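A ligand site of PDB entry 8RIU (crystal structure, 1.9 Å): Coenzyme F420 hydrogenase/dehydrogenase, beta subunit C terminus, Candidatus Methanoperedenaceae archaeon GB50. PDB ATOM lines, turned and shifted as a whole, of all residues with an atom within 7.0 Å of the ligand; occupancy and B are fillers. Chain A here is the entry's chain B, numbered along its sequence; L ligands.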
ATOM      1  N   LEU A  12      10.190  14.589 -14.946  1.00  0.00           N
ATOM      2  CA  LEU A  12      10.797  14.794 -16.262  1.00  0.00           C
ATOM      3  C   LEU A  12      11.416  13.518 -16.794  1.00  0.00           C
ATOM      4  O   LEU A  12      11.238  13.165 -17.963  1.00  0.00           O
ATOM      5  CB  LEU A  12      11.853  15.902 -16.174  1.00  0.00           C
ATOM      6  CG  LEU A  12      12.467  16.311 -17.506  1.00  0.00           C
ATOM      7  CD1 LEU A  12      11.406  16.948 -18.397  1.00  0.00           C
ATOM      8  CD2 LEU A  12      13.596  17.280 -17.256  1.00  0.00           C
ATOM      9  N   VAL A  16       9.586  11.975 -19.931  1.00  0.00           N
ATOM     10  CA  VAL A  16      10.209  12.521 -21.132  1.00  0.00           C
ATOM     11  C   VAL A  16      11.519  11.793 -21.423  1.00  0.00           C
ATOM     12  O   VAL A  16      11.646  11.127 -22.458  1.00  0.00           O
ATOM     13  CB  VAL A  16      10.432  14.036 -20.985  1.00  0.00           C
ATOM     14  CG1 VAL A  16      11.112  14.607 -22.224  1.00  0.00           C
ATOM     15  CG2 VAL A  16       9.106  14.736 -20.741  1.00  0.00           C
ATOM     16  N   VAL A  17      12.495  11.881 -20.524  1.00  0.00           N
ATOM     17  CA  VAL A  17      13.815  11.338 -20.806  1.00  0.00           C
ATOM     18  C   VAL A  17      13.748   9.833 -21.070  1.00  0.00           C
ATOM     19  O   VAL A  17      14.159   9.352 -22.130  1.00  0.00           O
ATOM     20  CB  VAL A  17      14.792  11.615 -19.642  1.00  0.00           C
ATOM     21  CG1 VAL A  17      16.189  11.112 -19.989  1.00  0.00           C
ATOM     22  CG2 VAL A  17      14.826  13.103 -19.325  1.00  0.00           C
ATOM     23  N   ILE A  21      11.281  10.745 -25.581  1.00  0.00           N
ATOM     24  CA  ILE A  21      10.661  11.840 -26.316  1.00  0.00           C
ATOM     25  C   ILE A  21      11.309  13.175 -26.008  1.00  0.00           C
ATOM     26  O   ILE A  21      10.742  14.228 -26.338  1.00  0.00           O
ATOM     27  CB  ILE A  21       9.136  11.896 -26.061  1.00  0.00           C
ATOM     28  CG1 ILE A  21       8.843  12.262 -24.601  1.00  0.00           C
ATOM     29  CG2 ILE A  21       8.491  10.563 -26.425  1.00  0.00           C
ATOM     30  CD1 ILE A  21       7.365  12.444 -24.313  1.00  0.00           C
ATOM     31  N   CYS A  22      12.496  13.186 -25.390  1.00  0.00           N
ATOM     32  CA  CYS A  22      13.254  14.426 -25.283  1.00  0.00           C
ATOM     33  C   CYS A  22      13.747  14.814 -26.673  1.00  0.00           C
ATOM     34  O   CYS A  22      14.307  13.986 -27.398  1.00  0.00           O
ATOM     35  CB  CYS A  22      14.437  14.266 -24.323  1.00  0.00           C
ATOM     36  SG  CYS A  22      15.639  15.661 -24.283  1.00  0.00           S
ATOM     37  N   CYS A  23      13.570  16.101 -27.021  1.00  0.00           N
ATOM     38  CA  CYS A  23      13.914  16.612 -28.378  1.00  0.00           C
ATOM     39  C   CYS A  23      15.169  17.484 -28.347  1.00  0.00           C
ATOM     40  O   CYS A  23      15.494  18.053 -29.394  1.00  0.00           O
ATOM     41  CB  CYS A  23      12.765  17.447 -28.931  1.00  0.00           C
ATOM     42  SG  CYS A  23      12.333  18.883 -27.917  1.00  0.00           S
ATOM     43  N   TYR A  24      15.833  17.598 -27.196  1.00  0.00           N
ATOM     44  CA  TYR A  24      17.101  18.364 -27.058  1.00  0.00           C
ATOM     45  C   TYR A  24      16.890  19.852 -27.350  1.00  0.00           C
ATOM     46  O   TYR A  24      17.749  20.463 -27.973  1.00  0.00           O
ATOM     47  CB  TYR A  24      18.224  17.711 -27.870  1.00  0.00           C
ATOM     48  CG  TYR A  24      19.619  18.152 -27.516  1.00  0.00           C
ATOM     49  CD1 TYR A  24      19.983  18.398 -26.210  1.00  0.00           C
ATOM     50  CD2 TYR A  24      20.577  18.302 -28.498  1.00  0.00           C
ATOM     51  CE1 TYR A  24      21.273  18.797 -25.882  1.00  0.00           C
ATOM     52  CE2 TYR A  24      21.871  18.700 -28.195  1.00  0.00           C
ATOM     53  CZ  TYR A  24      22.215  18.949 -26.879  1.00  0.00           C
ATOM     54  OH  TYR A  24      23.497  19.339 -26.586  1.00  0.00           O
ATOM     55  N   CYS A  25      15.788  20.420 -26.834  1.00  0.00           N
ATOM     56  CA  CYS A  25      15.469  21.860 -27.029  1.00  0.00           C
ATOM     57  C   CYS A  25      16.419  22.707 -26.180  1.00  0.00           C
ATOM     58  O   CYS A  25      16.683  23.843 -26.568  1.00  0.00           O
ATOM     59  CB  CYS A  25      14.023  22.126 -26.660  1.00  0.00           C
ATOM     60  SG  CYS A  25      13.676  22.146 -24.883  1.00  0.00           S
ATOM     61  N   GLY A  26      16.885  22.179 -25.052  1.00  0.00           N
ATOM     62  CA  GLY A  26      17.818  22.879 -24.197  1.00  0.00           C
ATOM     63  C   GLY A  26      17.210  23.633 -23.036  1.00  0.00           C
ATOM     64  O   GLY A  26      17.956  24.253 -22.265  1.00  0.00           O
ATOM     65  N   ALA A  27      15.889  23.586 -22.864  1.00  0.00           N
ATOM     66  CA  ALA A  27      15.231  24.474 -21.899  1.00  0.00           C
ATOM     67  C   ALA A  27      15.498  24.048 -20.464  1.00  0.00           C
ATOM     68  O   ALA A  27      15.726  24.889 -19.588  1.00  0.00           O
ATOM     69  CB  ALA A  27      13.733  24.533 -22.185  1.00  0.00           C
ATOM     70  N   CYS A  28      15.473  22.739 -20.186  1.00  0.00           N
ATOM     71  CA  CYS A  28      15.694  22.288 -18.819  1.00  0.00           C
ATOM     72  C   CYS A  28      17.099  22.647 -18.338  1.00  0.00           C
ATOM     73  O   CYS A  28      17.285  23.063 -17.185  1.00  0.00           O
ATOM     74  CB  CYS A  28      15.472  20.772 -18.718  1.00  0.00           C
ATOM     75  SG  CYS A  28      16.390  19.738 -19.905  1.00  0.00           S
ATOM     76  N   GLY A  29      18.098  22.507 -19.204  1.00  0.00           N
ATOM     77  CA  GLY A  29      19.450  22.864 -18.825  1.00  0.00           C
ATOM     78  C   GLY A  29      19.684  24.363 -18.768  1.00  0.00           C
ATOM     79  O   GLY A  29      20.482  24.842 -17.973  1.00  0.00           O
ATOM     80  N   ILE A  36      21.640  20.288 -13.978  1.00  0.00           N
ATOM     81  CA  ILE A  36      21.434  19.593 -15.234  1.00  0.00           C
ATOM     82  C   ILE A  36      22.634  19.821 -16.133  1.00  0.00           C
ATOM     83  O   ILE A  36      23.120  20.945 -16.278  1.00  0.00           O
ATOM     84  CB  ILE A  36      20.125  20.052 -15.910  1.00  0.00           C
ATOM     85  CG1 ILE A  36      18.924  19.468 -15.160  1.00  0.00           C
ATOM     86  CG2 ILE A  36      20.102  19.640 -17.377  1.00  0.00           C
ATOM     87  CD1 ILE A  36      17.581  19.729 -15.795  1.00  0.00           C
ATOM     88  N   TYR A  38      24.042  17.917 -20.131  1.00  0.00           N
ATOM     89  CA  TYR A  38      23.543  17.160 -21.263  1.00  0.00           C
ATOM     90  C   TYR A  38      24.549  16.103 -21.670  1.00  0.00           C
ATOM     91  O   TYR A  38      25.746  16.379 -21.762  1.00  0.00           O
ATOM     92  CB  TYR A  38      23.228  18.089 -22.449  1.00  0.00           C
ATOM     93  CG  TYR A  38      21.961  18.889 -22.264  1.00  0.00           C
ATOM     94  CD1 TYR A  38      20.718  18.274 -22.274  1.00  0.00           C
ATOM     95  CD2 TYR A  38      21.990  20.274 -22.102  1.00  0.00           C
ATOM     96  CE1 TYR A  38      19.556  18.994 -22.113  1.00  0.00           C
ATOM     97  CE2 TYR A  38      20.820  21.016 -21.942  1.00  0.00           C
ATOM     98  CZ  TYR A  38      19.610  20.364 -21.955  1.00  0.00           C
ATOM     99  OH  TYR A  38      18.444  21.069 -21.787  1.00  0.00           O
ATOM    100  N   GLY A  41      22.608  14.429 -25.922  1.00  0.00           N
ATOM    101  CA  GLY A  41      21.415  15.197 -26.196  1.00  0.00           C
ATOM    102  C   GLY A  41      20.265  14.967 -25.240  1.00  0.00           C
ATOM    103  O   GLY A  41      19.121  15.269 -25.583  1.00  0.00           O
ATOM    104  N   THR A  42      20.523  14.446 -24.035  1.00  0.00           N
ATOM    105  CA  THR A  42      19.459  14.294 -23.043  1.00  0.00           C
ATOM    106  C   THR A  42      19.951  14.766 -21.695  1.00  0.00           C
ATOM    107  O   THR A  42      21.129  14.593 -21.358  1.00  0.00           O
ATOM    108  CB  THR A  42      18.979  12.843 -22.927  1.00  0.00           C
ATOM    109  OG1 THR A  42      20.074  11.996 -22.558  1.00  0.00           O
ATOM    110  CG2 THR A  42      18.407  12.369 -24.254  1.00  0.00           C
ATOM    111  N   PRO A  43      19.077  15.357 -20.882  1.00  0.00           N
ATOM    112  CA  PRO A  43      19.514  15.901 -19.601  1.00  0.00           C
ATOM    113  C   PRO A  43      19.796  14.812 -18.578  1.00  0.00           C
ATOM    114  O   PRO A  43      19.097  13.799 -18.512  1.00  0.00           O
ATOM    115  CB  PRO A  43      18.332  16.782 -19.167  1.00  0.00           C
ATOM    116  CG  PRO A  43      17.154  16.145 -19.831  1.00  0.00           C
ATOM    117  CD  PRO A  43      17.648  15.613 -21.134  1.00  0.00           C
ATOM    118  N   ALA A  55      11.811  23.996 -12.615  1.00  0.00           N
ATOM    119  CA  ALA A  55      11.687  24.617 -13.922  1.00  0.00           C
ATOM    120  C   ALA A  55      11.952  23.613 -15.033  1.00  0.00           C
ATOM    121  O   ALA A  55      11.401  23.750 -16.127  1.00  0.00           O
ATOM    122  CB  ALA A  55      12.643  25.808 -14.037  1.00  0.00           C
ATOM    123  N   CYS A  56      12.796  22.612 -14.779  1.00  0.00           N
ATOM    124  CA  CYS A  56      13.067  21.589 -15.785  1.00  0.00           C
ATOM    125  C   CYS A  56      11.773  20.981 -16.303  1.00  0.00           C
ATOM    126  O   CYS A  56      11.583  20.829 -17.515  1.00  0.00           O
ATOM    127  CB  CYS A  56      13.977  20.501 -15.203  1.00  0.00           C
ATOM    128  SG  CYS A  56      13.318  19.603 -13.739  1.00  0.00           S
ATOM    129  N   PHE A  57      10.857  20.661 -15.393  1.00  0.00           N
ATOM    130  CA  PHE A  57       9.585  20.080 -15.775  1.00  0.00           C
ATOM    131  C   PHE A  57       8.623  21.139 -16.311  1.00  0.00           C
ATOM    132  O   PHE A  57       7.871  20.883 -17.257  1.00  0.00           O
ATOM    133  CB  PHE A  57       8.961  19.369 -14.571  1.00  0.00           C
ATOM    134  CG  PHE A  57       7.646  18.708 -14.859  1.00  0.00           C
ATOM    135  CD1 PHE A  57       7.600  17.413 -15.335  1.00  0.00           C
ATOM    136  CD2 PHE A  57       6.465  19.385 -14.625  1.00  0.00           C
ATOM    137  CE1 PHE A  57       6.387  16.804 -15.593  1.00  0.00           C
ATOM    138  CE2 PHE A  57       5.247  18.788 -14.888  1.00  0.00           C
ATOM    139  CZ  PHE A  57       5.210  17.496 -15.367  1.00  0.00           C
ATOM    140  N   PHE A  59       9.236  23.986 -17.909  1.00  0.00           N
ATOM    141  CA  PHE A  59       9.594  24.592 -19.195  1.00  0.00           C
ATOM    142  C   PHE A  59       9.664  23.586 -20.338  1.00  0.00           C
ATOM    143  O   PHE A  59       9.752  23.992 -21.498  1.00  0.00           O
ATOM    144  CB  PHE A  59      10.946  25.308 -19.085  1.00  0.00           C
ATOM    145  CG  PHE A  59      10.948  26.510 -18.180  1.00  0.00           C
ATOM    146  CD1 PHE A  59       9.755  27.019 -17.668  1.00  0.00           C
ATOM    147  CD2 PHE A  59      12.135  27.130 -17.852  1.00  0.00           C
ATOM    148  CE1 PHE A  59       9.776  28.123 -16.836  1.00  0.00           C
ATOM    149  CE2 PHE A  59      12.157  28.234 -17.020  1.00  0.00           C
ATOM    150  CZ  PHE A  59      10.974  28.736 -16.514  1.00  0.00           C
ATOM    151  N   CYS A  60       9.639  22.293 -20.044  1.00  0.00           N
ATOM    152  CA  CYS A  60       9.857  21.298 -21.087  1.00  0.00           C
ATOM    153  C   CYS A  60       8.638  21.220 -22.018  1.00  0.00           C
ATOM    154  O   CYS A  60       7.507  21.118 -21.537  1.00  0.00           O
ATOM    155  CB  CYS A  60      10.113  19.934 -20.457  1.00  0.00           C
ATOM    156  SG  CYS A  60      10.216  18.593 -21.621  1.00  0.00           S
ATOM    157  N   PRO A  61       8.833  21.271 -23.336  1.00  0.00           N
ATOM    158  CA  PRO A  61       7.686  21.180 -24.256  1.00  0.00           C
ATOM    159  C   PRO A  61       7.082  19.787 -24.341  1.00  0.00           C
ATOM    160  O   PRO A  61       6.063  19.628 -25.031  1.00  0.00           O
ATOM    161  CB  PRO A  61       8.280  21.596 -25.611  1.00  0.00           C
ATOM    162  CG  PRO A  61       9.713  21.175 -25.517  1.00  0.00           C
ATOM    163  CD  PRO A  61      10.119  21.393 -24.068  1.00  0.00           C
ATOM    164  N   ARG A  62       7.670  18.783 -23.688  1.00  0.00           N
ATOM    165  CA  ARG A  62       7.210  17.412 -23.814  1.00  0.00           C
ATOM    166  C   ARG A  62       6.597  16.847 -22.533  1.00  0.00           C
ATOM    167  O   ARG A  62       6.203  15.683 -22.518  1.00  0.00           O
ATOM    168  CB  ARG A  62       8.381  16.522 -24.259  1.00  0.00           C
ATOM    169  CG  ARG A  62       8.865  16.801 -25.680  1.00  0.00           C
ATOM    170  CD  ARG A  62       7.912  16.251 -26.727  1.00  0.00           C
ATOM    171  NE  ARG A  62       8.173  16.811 -28.055  1.00  0.00           N
ATOM    172  CZ  ARG A  62       9.038  16.321 -28.933  1.00  0.00           C
ATOM    173  NH1 ARG A  62       9.769  15.255 -28.653  1.00  0.00           N
ATOM    174  NH2 ARG A  62       9.179  16.928 -30.107  1.00  0.00           N
ATOM    175  N   THR A  63       6.485  17.634 -21.465  1.00  0.00           N
ATOM    176  CA  THR A  63       5.770  17.204 -20.268  1.00  0.00           C
ATOM    177  C   THR A  63       4.286  17.541 -20.368  1.00  0.00           C
ATOM    178  O   THR A  63       3.431  16.670 -20.238  1.00  0.00           O
ATOM    179  CB  THR A  63       6.378  17.836 -19.018  1.00  0.00           C
ATOM    180  OG1 THR A  63       6.444  19.262 -19.185  1.00  0.00           O
ATOM    181  CG2 THR A  63       7.770  17.280 -18.769  1.00  0.00           C
ATOM    182  N   PRO A 162      20.733  22.815 -28.793  1.00  0.00           N
ATOM    183  CA  PRO A 162      20.011  23.160 -27.569  1.00  0.00           C
ATOM    184  C   PRO A 162      19.911  24.693 -27.565  1.00  0.00           C
ATOM    185  O   PRO A 162      20.469  25.315 -26.693  1.00  0.00           O
ATOM    186  CB  PRO A 162      20.933  22.620 -26.465  1.00  0.00           C
ATOM    187  CG  PRO A 162      22.316  22.699 -27.070  1.00  0.00           C
ATOM    188  CD  PRO A 162      22.125  22.433 -28.544  1.00  0.00           C
ATOM    189  N   ILE A 164      17.755  26.840 -26.658  1.00  0.00           N
ATOM    190  CA  ILE A 164      17.260  27.557 -25.488  1.00  0.00           C
ATOM    191  C   ILE A 164      18.395  27.824 -24.495  1.00  0.00           C
ATOM    192  O   ILE A 164      18.269  28.718 -23.646  1.00  0.00           O
ATOM    193  CB  ILE A 164      16.100  26.795 -24.822  1.00  0.00           C
ATOM    194  CG1 ILE A 164      15.010  26.461 -25.844  1.00  0.00           C
ATOM    195  CG2 ILE A 164      15.510  27.588 -23.667  1.00  0.00           C
ATOM    196  CD1 ILE A 164      14.402  27.681 -26.555  1.00  0.00           C
ATOM    197  N   CYS A 185      10.092  23.018 -31.846  1.00  0.00           N
ATOM    198  CA  CYS A 185      10.214  22.577 -30.469  1.00  0.00           C
ATOM    199  C   CYS A 185      10.847  23.659 -29.593  1.00  0.00           C
ATOM    200  O   CYS A 185      10.430  23.856 -28.453  1.00  0.00           O
ATOM    201  CB  CYS A 185      11.017  21.272 -30.409  1.00  0.00           C
ATOM    202  SG  CYS A 185      12.592  21.286 -31.306  1.00  0.00           S
ATOM    203  N   ALA A 189       9.076  25.508 -26.287  1.00  0.00           N
ATOM    204  CA  ALA A 189       9.730  25.719 -24.999  1.00  0.00           C
ATOM    205  C   ALA A 189       9.804  27.197 -24.667  1.00  0.00           C
ATOM    206  O   ALA A 189       9.574  27.604 -23.526  1.00  0.00           O
ATOM    207  CB  ALA A 189      11.120  25.096 -24.997  1.00  0.00           C
HETATM  208 FE1  LIG L   1      14.506  17.446 -23.408  1.00  0.00          FE
HETATM  209 FE2  LIG L   1      14.855  19.223 -21.479  1.00  0.00          FE
HETATM  210 FE3  LIG L   1      12.397  18.606 -22.227  1.00  0.00          FE
HETATM  211 FE4  LIG L   1      13.941  20.063 -23.901  1.00  0.00          FE
HETATM  212  S1  LIG L   1      13.157  20.679 -21.797  1.00  0.00           S
HETATM  213  S2  LIG L   1      12.648  18.227 -24.464  1.00  0.00           S
HETATM  214  S3  LIG L   1      16.031  19.172 -23.440  1.00  0.00           S
HETATM  215  S4  LIG L   1      13.863  17.173 -21.230  1.00  0.00           S
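S2 of the ligand sits close to SG of Cys 23, 3.5 Å away. A sulfur (S1) of the ligand lies close to the backbone NH (N) of Cys 28, 3.5 Å away. An iron atom (FE2) of the ligand is bound by the side-chain sulfur (SG) of Cys 28 (2.3 Å). The side-chain sulfur (SG) of Cys 22 binds an iron atom (FE1) of the ligand, at 2.3 Å. SG of Cys 60 is bound to FE3 of the ligand, at 2.3 Å. A sulfur (S3) of the ligand sits close to the backbone NH of Cys 25 (3.6 Å). N of Gly 26 sits close to S3 of the ligand (3.5 Å). The side-chain hydroxyl (OH) of Tyr 38 sits close to a sulfur (S3) of the ligand, at 3.5 Å. The backbone NH of Cys 23 sits close to a sulfur (S2) of the ligand, 3.5 Å away. FE4 of the ligand is bound by SG of Cys 25 (2.3 Å).
The side-chain hydroxyl of Tyr 38 lies close to the side-chain sulfur of Cys 28 (3.1 Å). N of Ile 164 lies within hydrogen-bond range of O of Cys 25, 3.2 Å away. The side-chain sulfur (SG) of Cys 25 sits close to the backbone NH (N) of Ala 27, 3.3 Å away. The side-chain sulfur (SG) of Cys 22 sits close to the backbone NH (N) of Tyr 24 (3.5 Å). The side-chain hydroxyl (OG1) of Thr 63 is in hydrogen-bond range of the backbone carbonyl oxygen (O) of Cys 60 (3.2 Å). The side-chain sulfur (SG) of Cys 60 lies close to the backbone NH (N) of Arg 62 (3.3 Å). O of Val 16 is in hydrogen-bond range of N of Ile 21, 3.2 Å away. OH of Tyr 38 sits at hydrogen-bond distance from N of Gly 29.
CD1 of Leu 12 touches S4 of the ligand, 3.8 Å away. Val 16 touches the ligand. CA of Tyr 24 touches S3 of the ligand, at 3.9 Å. CB of Ala 27 touches S1 of the ligand, 3.9 Å away. Pro 43 touches the ligand (CG to S4, 3.7 Å). Pro 61 touches the ligand. Hydrophobic or aromatic side chains within 4 Å of the ligand: Leu 12, Val 16, Ala 27, Tyr 38, Pro 43 and Pro 61. The nearest printed residue that does not touch the ligand is Arg 62 (4.2 Å).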
